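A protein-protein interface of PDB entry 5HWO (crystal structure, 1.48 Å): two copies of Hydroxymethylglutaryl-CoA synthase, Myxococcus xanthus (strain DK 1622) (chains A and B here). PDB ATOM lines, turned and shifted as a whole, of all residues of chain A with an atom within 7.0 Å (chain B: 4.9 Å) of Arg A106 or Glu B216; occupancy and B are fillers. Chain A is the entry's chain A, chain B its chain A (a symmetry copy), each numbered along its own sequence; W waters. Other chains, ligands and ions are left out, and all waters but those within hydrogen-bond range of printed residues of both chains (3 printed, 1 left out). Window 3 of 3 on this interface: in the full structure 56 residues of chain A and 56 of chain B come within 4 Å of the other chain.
O of Gln A99 lies within hydrogen-bond range of N of Leu A104 (3.0 Å).
The side-chain amide nitrogen (NE2) of Gln A99 lies within hydrogen-bond range of the backbone carbonyl oxygen (O) of Pro A105 (3.1 Å).
SD of Met A108 sits close to NE2 of Gln A99 (3.7 Å).
The side-chain amide nitrogen (NE2) of Gln A99 lies within hydrogen-bond range of the side-chain hydroxyl (OG) of Ser B188 (2.9 Å).
OE1 of Gln A99 lies close to N of Met B189, at 3.4 Å.
O of Arg A106 sits at hydrogen-bond distance from N of Ser B188 (2.9 Å).
The guanidinium group of Arg A106 lies within salt-bridge range of the side-chain carboxylate of Glu B216, at 2.7 Å.
The backbone carbonyl oxygen (O) of Met A108 is in hydrogen-bond range of the side-chain hydroxyl (OG) of Ser B188 (2.7 Å).
Arg A106 touches just these residues of chain B: Val B186 (3.8 Å), Cys B187 (3.2 Å), Ser B188 (2.9 Å), Met B189 (3.7 Å) and Glu B216 (2.7 Å).
Printed residues of chain B within 4 Å of Met A108: Val B186 (3.5 Å) and Ser B188 (2.7 Å).
Printed residues of chain B within 4 Å of Thr A110: Ser B188.
Tyr B214 touches none of the printed residues of chain A.
Glu B216 touches just one residue of chain A: Arg A106 (2.7 Å).
The nearest printed residue of chain B that does not touch Arg A106 is Ala B217 (6.1 Å).
Among the printed residues, merely in contact across the chains: Arg A106 with Cys B187 (3.2 Å), Met A108 with Val B186 (3.5 Å), Thr A107 with Val B186 (3.6 Å), Arg A106 with Met B189 (3.7 Å), Arg A106 with Val B186 (3.8 Å), Arg A109 with Val B186 (3.8 Å) and Thr A110 with Ser B188 (3.8 Å).
Of the 9 printed residues of chain A, 6 touch a printed residue of chain B.
Hydrophobic or aromatic side chains of chain A within 4 Å of the printed part of chain B: Met A108.
Of the 13 printed residues of chain B, 5 touch a printed residue of chain A.
Printed residues of chain B that touch a printed residue of chain A: Val B186, Cys B187, Ser B188, Met B189 and Glu B216.
Among the printed residues, Asp or Glu carboxylates within 4 Å of a Lys or Arg side-chain nitrogen of the other chain: Arg A106 with Glu B216.
No position is printed for both chains.
Of the 12 pairs that touch across the chains among the printed residues, none has its exchanged pair printed and touching as well.
Water W2 bridges O of Val B186 and OG1 of Thr A107.
Water W1 lies within hydrogen-bond range of the side-chain carboxylate of Glu B216 (2.8 Å) and the guanidinium group of Arg A106 (3.3 Å).
Water W3 lies within hydrogen-bond range of NH1 of Arg A106 (2.9 Å) and SG of Cys B187 (3.7 Å).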
ATOM      1  N   ILE A  77      20.183  -8.245 -28.828  1.00  0.00           N
ATOM      2  CA  ILE A  77      20.732  -9.520 -28.383  1.00  0.00           C
ATOM      3  C   ILE A  77      19.594 -10.343 -27.784  1.00  0.00           C
ATOM      4  O   ILE A  77      18.983  -9.938 -26.786  1.00  0.00           O
ATOM      5  CB  ILE A  77      21.851  -9.303 -27.355  1.00  0.00           C
ATOM      6  CG1 ILE A  77      22.998  -8.470 -27.957  1.00  0.00           C
ATOM      7  CG2 ILE A  77      22.344 -10.652 -26.816  1.00  0.00           C
ATOM      8  CD1 ILE A  77      23.992  -7.998 -26.950  1.00  0.00           C
ATOM      9  N   GLN A  99      25.816 -10.474 -18.343  1.00  0.00           N
ATOM     10  CA  GLN A  99      24.638  -9.644 -18.596  1.00  0.00           C
ATOM     11  C   GLN A  99      24.576  -8.477 -17.630  1.00  0.00           C
ATOM     12  O   GLN A  99      24.324  -7.341 -18.036  1.00  0.00           O
ATOM     13  CB  GLN A  99      23.381 -10.487 -18.451  1.00  0.00           C
ATOM     14  CG  GLN A  99      22.094  -9.718 -18.687  1.00  0.00           C
ATOM     15  CD  GLN A  99      20.873 -10.572 -18.514  1.00  0.00           C
ATOM     16  OE1 GLN A  99      20.765 -11.368 -17.587  1.00  0.00           O
ATOM     17  NE2 GLN A  99      19.950 -10.426 -19.412  1.00  0.00           N
ATOM     18  N   LEU A 104      23.111  -5.215 -19.715  1.00  0.00           N
ATOM     19  CA  LEU A 104      22.300  -5.594 -20.843  1.00  0.00           C
ATOM     20  C   LEU A 104      20.833  -5.706 -20.445  1.00  0.00           C
ATOM     21  O   LEU A 104      20.518  -6.016 -19.298  1.00  0.00           O
ATOM     22  CB  LEU A 104      22.744  -6.934 -21.396  1.00  0.00           C
ATOM     23  CG  LEU A 104      24.174  -7.019 -21.939  1.00  0.00           C
ATOM     24  CD1 LEU A 104      24.483  -8.454 -22.471  1.00  0.00           C
ATOM     25  CD2 LEU A 104      24.388  -5.985 -23.045  1.00  0.00           C
ATOM     26  N   PRO A 105      19.927  -5.489 -21.399  1.00  0.00           N
ATOM     27  CA  PRO A 105      18.488  -5.602 -21.117  1.00  0.00           C
ATOM     28  C   PRO A 105      18.017  -7.048 -21.000  1.00  0.00           C
ATOM     29  O   PRO A 105      18.828  -7.985 -20.994  1.00  0.00           O
ATOM     30  CB  PRO A 105      17.846  -4.836 -22.285  1.00  0.00           C
ATOM     31  CG  PRO A 105      18.837  -4.954 -23.417  1.00  0.00           C
ATOM     32  CD  PRO A 105      20.198  -5.003 -22.761  1.00  0.00           C
ATOM     33  N   ARG A 106      16.714  -7.231 -20.866  1.00  0.00           N
ATOM     34  CA  ARG A 106      16.155  -8.459 -20.315  1.00  0.00           C
ATOM     35  C   ARG A 106      15.685  -9.477 -21.339  1.00  0.00           C
ATOM     36  O   ARG A 106      15.453 -10.631 -20.960  1.00  0.00           O
ATOM     37  CB  ARG A 106      14.985  -8.138 -19.369  1.00  0.00           C
ATOM     38  CG  ARG A 106      15.429  -7.395 -18.123  1.00  0.00           C
ATOM     39  CD  ARG A 106      14.285  -7.080 -17.180  1.00  0.00           C
ATOM     40  NE  ARG A 106      14.825  -6.637 -15.906  1.00  0.00           N
ATOM     41  CZ  ARG A 106      14.146  -6.601 -14.777  1.00  0.00           C
ATOM     42  NH1 ARG A 106      12.864  -6.931 -14.752  1.00  0.00           N
ATOM     43  NH2 ARG A 106      14.785  -6.252 -13.663  1.00  0.00           N
ATOM     44  N   THR A 107      15.510  -9.096 -22.599  1.00  0.00           N
ATOM     45  CA  THR A 107      14.852  -9.986 -23.555  1.00  0.00           C
ATOM     46  C   THR A 107      15.870 -10.874 -24.264  1.00  0.00           C
ATOM     47  O   THR A 107      16.052 -10.842 -25.481  1.00  0.00           O
ATOM     48  CB  THR A 107      13.985  -9.208 -24.534  1.00  0.00           C
ATOM     49  OG1 THR A 107      13.210  -8.228 -23.825  1.00  0.00           O
ATOM     50  CG2 THR A 107      13.067 -10.189 -25.259  1.00  0.00           C
ATOM     51  N   MET A 108      16.512 -11.716 -23.450  1.00  0.00           N
ATOM     52  CA  MET A 108      17.451 -12.690 -23.979  1.00  0.00           C
ATOM     53  C   MET A 108      17.488 -13.944 -23.104  1.00  0.00           C
ATOM     54  O   MET A 108      17.329 -13.887 -21.882  1.00  0.00           O
ATOM     55  CB  MET A 108      18.868 -12.100 -24.070  1.00  0.00           C
ATOM     56  CG  MET A 108      19.409 -11.548 -22.739  1.00  0.00           C
ATOM     57  SD  MET A 108      21.012 -10.718 -22.945  1.00  0.00           S
ATOM     58  CE  MET A 108      20.512  -9.254 -23.774  1.00  0.00           C
ATOM     59  N   ARG A 109      17.740 -15.078 -23.757  1.00  0.00           N
ATOM     60  CA  ARG A 109      18.161 -16.282 -23.042  1.00  0.00           C
ATOM     61  C   ARG A 109      19.578 -16.069 -22.527  1.00  0.00           C
ATOM     62  O   ARG A 109      20.414 -15.498 -23.224  1.00  0.00           O
ATOM     63  CB  ARG A 109      18.174 -17.493 -23.980  1.00  0.00           C
ATOM     64  CG  ARG A 109      16.875 -17.869 -24.646  1.00  0.00           C
ATOM     65  CD  ARG A 109      17.024 -19.124 -25.479  1.00  0.00           C
ATOM     66  NE  ARG A 109      15.809 -19.385 -26.222  1.00  0.00           N
ATOM     67  CZ  ARG A 109      15.735 -20.014 -27.377  1.00  0.00           C
ATOM     68  NH1 ARG A 109      16.813 -20.504 -27.969  1.00  0.00           N
ATOM     69  NH2 ARG A 109      14.549 -20.141 -27.944  1.00  0.00           N
ATOM     70  N   THR A 110      19.858 -16.541 -21.311  1.00  0.00           N
ATOM     71  CA  THR A 110      21.224 -16.593 -20.792  1.00  0.00           C
ATOM     72  C   THR A 110      21.497 -17.987 -20.242  1.00  0.00           C
ATOM     73  O   THR A 110      20.661 -18.550 -19.538  1.00  0.00           O
ATOM     74  CB  THR A 110      21.480 -15.570 -19.677  1.00  0.00           C
ATOM     75  OG1 THR A 110      20.587 -15.818 -18.588  1.00  0.00           O
ATOM     76  CG2 THR A 110      21.280 -14.144 -20.154  1.00  0.00           C
ATOM     77  N   VAL B 186      10.911 -14.217 -23.169  1.00  0.00           N
ATOM     78  CA  VAL B 186      12.047 -14.436 -22.283  1.00  0.00           C
ATOM     79  C   VAL B 186      12.322 -13.172 -21.466  1.00  0.00           C
ATOM     80  O   VAL B 186      12.112 -12.042 -21.926  1.00  0.00           O
ATOM     81  CB  VAL B 186      13.272 -14.941 -23.091  1.00  0.00           C
ATOM     82  CG1 VAL B 186      13.809 -13.836 -23.976  1.00  0.00           C
ATOM     83  CG2 VAL B 186      14.327 -15.595 -22.200  1.00  0.00           C
ATOM     84  N   CYS B 187      12.786 -13.372 -20.233  1.00  0.00           N
ATOM     85  CA  CYS B 187      13.148 -12.259 -19.357  1.00  0.00           C
ATOM     86  C   CYS B 187      14.253 -12.724 -18.425  1.00  0.00           C
ATOM     87  O   CYS B 187      14.067 -13.687 -17.676  1.00  0.00           O
ATOM     88  CB  CYS B 187      11.925 -11.861 -18.539  1.00  0.00           C
ATOM     89  SG  CYS B 187      12.226 -10.446 -17.443  1.00  0.00           S
ATOM     90  N   SER B 188      15.384 -12.037 -18.459  1.00  0.00           N
ATOM     91  CA  SER B 188      16.547 -12.428 -17.683  1.00  0.00           C
ATOM     92  C   SER B 188      17.245 -11.200 -17.114  1.00  0.00           C
ATOM     93  O   SER B 188      17.305 -10.140 -17.746  1.00  0.00           O
ATOM     94  CB  SER B 188      17.518 -13.254 -18.549  1.00  0.00           C
ATOM     95  OG  SER B 188      17.908 -12.476 -19.675  1.00  0.00           O
ATOM     96  N   MET B 189      17.778 -11.358 -15.915  1.00  0.00           N
ATOM     97  CA  MET B 189      18.564 -10.303 -15.293  1.00  0.00           C
ATOM     98  C   MET B 189      19.457 -10.914 -14.230  1.00  0.00           C
ATOM     99  O   MET B 189      19.133 -11.954 -13.650  1.00  0.00           O
ATOM    100  CB  MET B 189      17.698  -9.191 -14.691  1.00  0.00           C
ATOM    101  CG  MET B 189      16.669  -9.656 -13.709  1.00  0.00           C
ATOM    102  SD  MET B 189      15.137 -10.200 -14.449  1.00  0.00           S
ATOM    103  CE  MET B 189      14.090 -10.279 -12.987  1.00  0.00           C
ATOM    104  N   THR B 212       9.933 -13.397  -5.401  1.00  0.00           N
ATOM    105  CA  THR B 212       9.716 -12.164  -6.151  1.00  0.00           C
ATOM    106  C   THR B 212      10.421 -12.209  -7.495  1.00  0.00           C
ATOM    107  O   THR B 212       9.850 -11.784  -8.509  1.00  0.00           O
ATOM    108  CB  THR B 212      10.149 -10.964  -5.325  1.00  0.00           C
ATOM    109  OG1 THR B 212       9.392 -10.955  -4.113  1.00  0.00           O
ATOM    110  CG2 THR B 212       9.911  -9.658  -6.091  1.00  0.00           C
ATOM    111  N   CYS B 213      11.658 -12.739  -7.535  1.00  0.00           N
ATOM    112  CA  CYS B 213      12.383 -12.808  -8.807  1.00  0.00           C
ATOM    113  C   CYS B 213      11.685 -13.741  -9.785  1.00  0.00           C
ATOM    114  O   CYS B 213      11.566 -13.422 -10.966  1.00  0.00           O
ATOM    115  CB  CYS B 213      13.842 -13.221  -8.616  1.00  0.00           C
ATOM    116  SG  CYS B 213      14.871 -11.964  -7.801  1.00  0.00           S
ATOM    117  N   TYR B 214      11.238 -14.912  -9.327  1.00  0.00           N
ATOM    118  CA  TYR B 214      10.482 -15.814 -10.191  1.00  0.00           C
ATOM    119  C   TYR B 214       9.295 -15.088 -10.800  1.00  0.00           C
ATOM    120  O   TYR B 214       9.074 -15.144 -12.007  1.00  0.00           O
ATOM    121  CB  TYR B 214      10.049 -17.025  -9.348  1.00  0.00           C
ATOM    122  CG  TYR B 214       9.218 -18.130  -9.976  1.00  0.00           C
ATOM    123  CD1 TYR B 214       8.078 -17.867 -10.713  1.00  0.00           C
ATOM    124  CD2 TYR B 214       9.535 -19.447  -9.746  1.00  0.00           C
ATOM    125  CE1 TYR B 214       7.304 -18.891 -11.242  1.00  0.00           C
ATOM    126  CE2 TYR B 214       8.750 -20.488 -10.258  1.00  0.00           C
ATOM    127  CZ  TYR B 214       7.648 -20.200 -11.000  1.00  0.00           C
ATOM    128  OH  TYR B 214       6.845 -21.181 -11.533  1.00  0.00           O
ATOM    129  N   LEU B 215       8.500 -14.417  -9.962  1.00  0.00           N
ATOM    130  CA  LEU B 215       7.286 -13.777 -10.453  1.00  0.00           C
ATOM    131  C   LEU B 215       7.604 -12.618 -11.393  1.00  0.00           C
ATOM    132  O   LEU B 215       6.893 -12.405 -12.376  1.00  0.00           O
ATOM    133  CB  LEU B 215       6.397 -13.354  -9.287  1.00  0.00           C
ATOM    134  CG  LEU B 215       5.908 -14.511  -8.420  1.00  0.00           C
ATOM    135  CD1 LEU B 215       5.137 -14.023  -7.223  1.00  0.00           C
ATOM    136  CD2 LEU B 215       5.070 -15.528  -9.205  1.00  0.00           C
ATOM    137  N   GLU B 216       8.660 -11.852 -11.106  1.00  0.00           N
ATOM    138  CA  GLU B 216       9.050 -10.759 -11.989  1.00  0.00           C
ATOM    139  C   GLU B 216       9.472 -11.286 -13.349  1.00  0.00           C
ATOM    140  O   GLU B 216       9.038 -10.776 -14.393  1.00  0.00           O
ATOM    141  CB  GLU B 216      10.196  -9.951 -11.355  1.00  0.00           C
ATOM    142  CG  GLU B 216      10.627  -8.773 -12.183  1.00  0.00           C
ATOM    143  CD  GLU B 216      11.720  -7.923 -11.572  1.00  0.00           C
ATOM    144  OE1 GLU B 216      12.320  -8.297 -10.530  1.00  0.00           O
ATOM    145  OE2 GLU B 216      11.977  -6.840 -12.166  1.00  0.00           O
ATOM    146  N   ALA B 217      10.355 -12.285 -13.359  1.00  0.00           N
ATOM    147  CA  ALA B 217      10.811 -12.850 -14.625  1.00  0.00           C
ATOM    148  C   ALA B 217       9.671 -13.535 -15.364  1.00  0.00           C
ATOM    149  O   ALA B 217       9.554 -13.418 -16.594  1.00  0.00           O
ATOM    150  CB  ALA B 217      11.982 -13.811 -14.401  1.00  0.00           C
ATOM    151  N   LEU B 218       8.808 -14.246 -14.637  1.00  0.00           N
ATOM    152  CA  LEU B 218       7.625 -14.827 -15.271  1.00  0.00           C
ATOM    153  C   LEU B 218       6.813 -13.760 -15.996  1.00  0.00           C
ATOM    154  O   LEU B 218       6.357 -13.970 -17.130  1.00  0.00           O
ATOM    155  CB  LEU B 218       6.763 -15.529 -14.212  1.00  0.00           C
ATOM    156  CG  LEU B 218       5.375 -16.019 -14.639  1.00  0.00           C
ATOM    157  CD1 LEU B 218       4.944 -17.112 -13.647  1.00  0.00           C
ATOM    158  CD2 LEU B 218       4.293 -14.950 -14.679  1.00  0.00           C
ATOM    159  N   SER B 219       6.582 -12.625 -15.330  1.00  0.00           N
ATOM    160  CA  SER B 219       5.753 -11.579 -15.915  1.00  0.00           C
ATOM    161  C   SER B 219       6.327 -11.113 -17.246  1.00  0.00           C
ATOM    162  O   SER B 219       5.589 -10.926 -18.218  1.00  0.00           O
ATOM    163  CB  SER B 219       5.648 -10.398 -14.942  1.00  0.00           C
ATOM    164  OG  SER B 219       4.980 -10.758 -13.749  1.00  0.00           O
ATOM    165  N   GLY B 220       7.639 -10.871 -17.290  1.00  0.00           N
ATOM    166  CA  GLY B 220       8.255 -10.440 -18.532  1.00  0.00           C
ATOM    167  C   GLY B 220       8.217 -11.504 -19.616  1.00  0.00           C
ATOM    168  O   GLY B 220       7.957 -11.209 -20.797  1.00  0.00           O
HETATM  169  O   HOH W   1      14.811  -7.061 -10.469  1.00  0.00           O
HETATM  170  O   HOH W   2      11.874  -9.427 -21.449  1.00  0.00           O
HETATM  171  O   HOH W   3      10.847  -7.078 -16.855  1.00  0.00           O
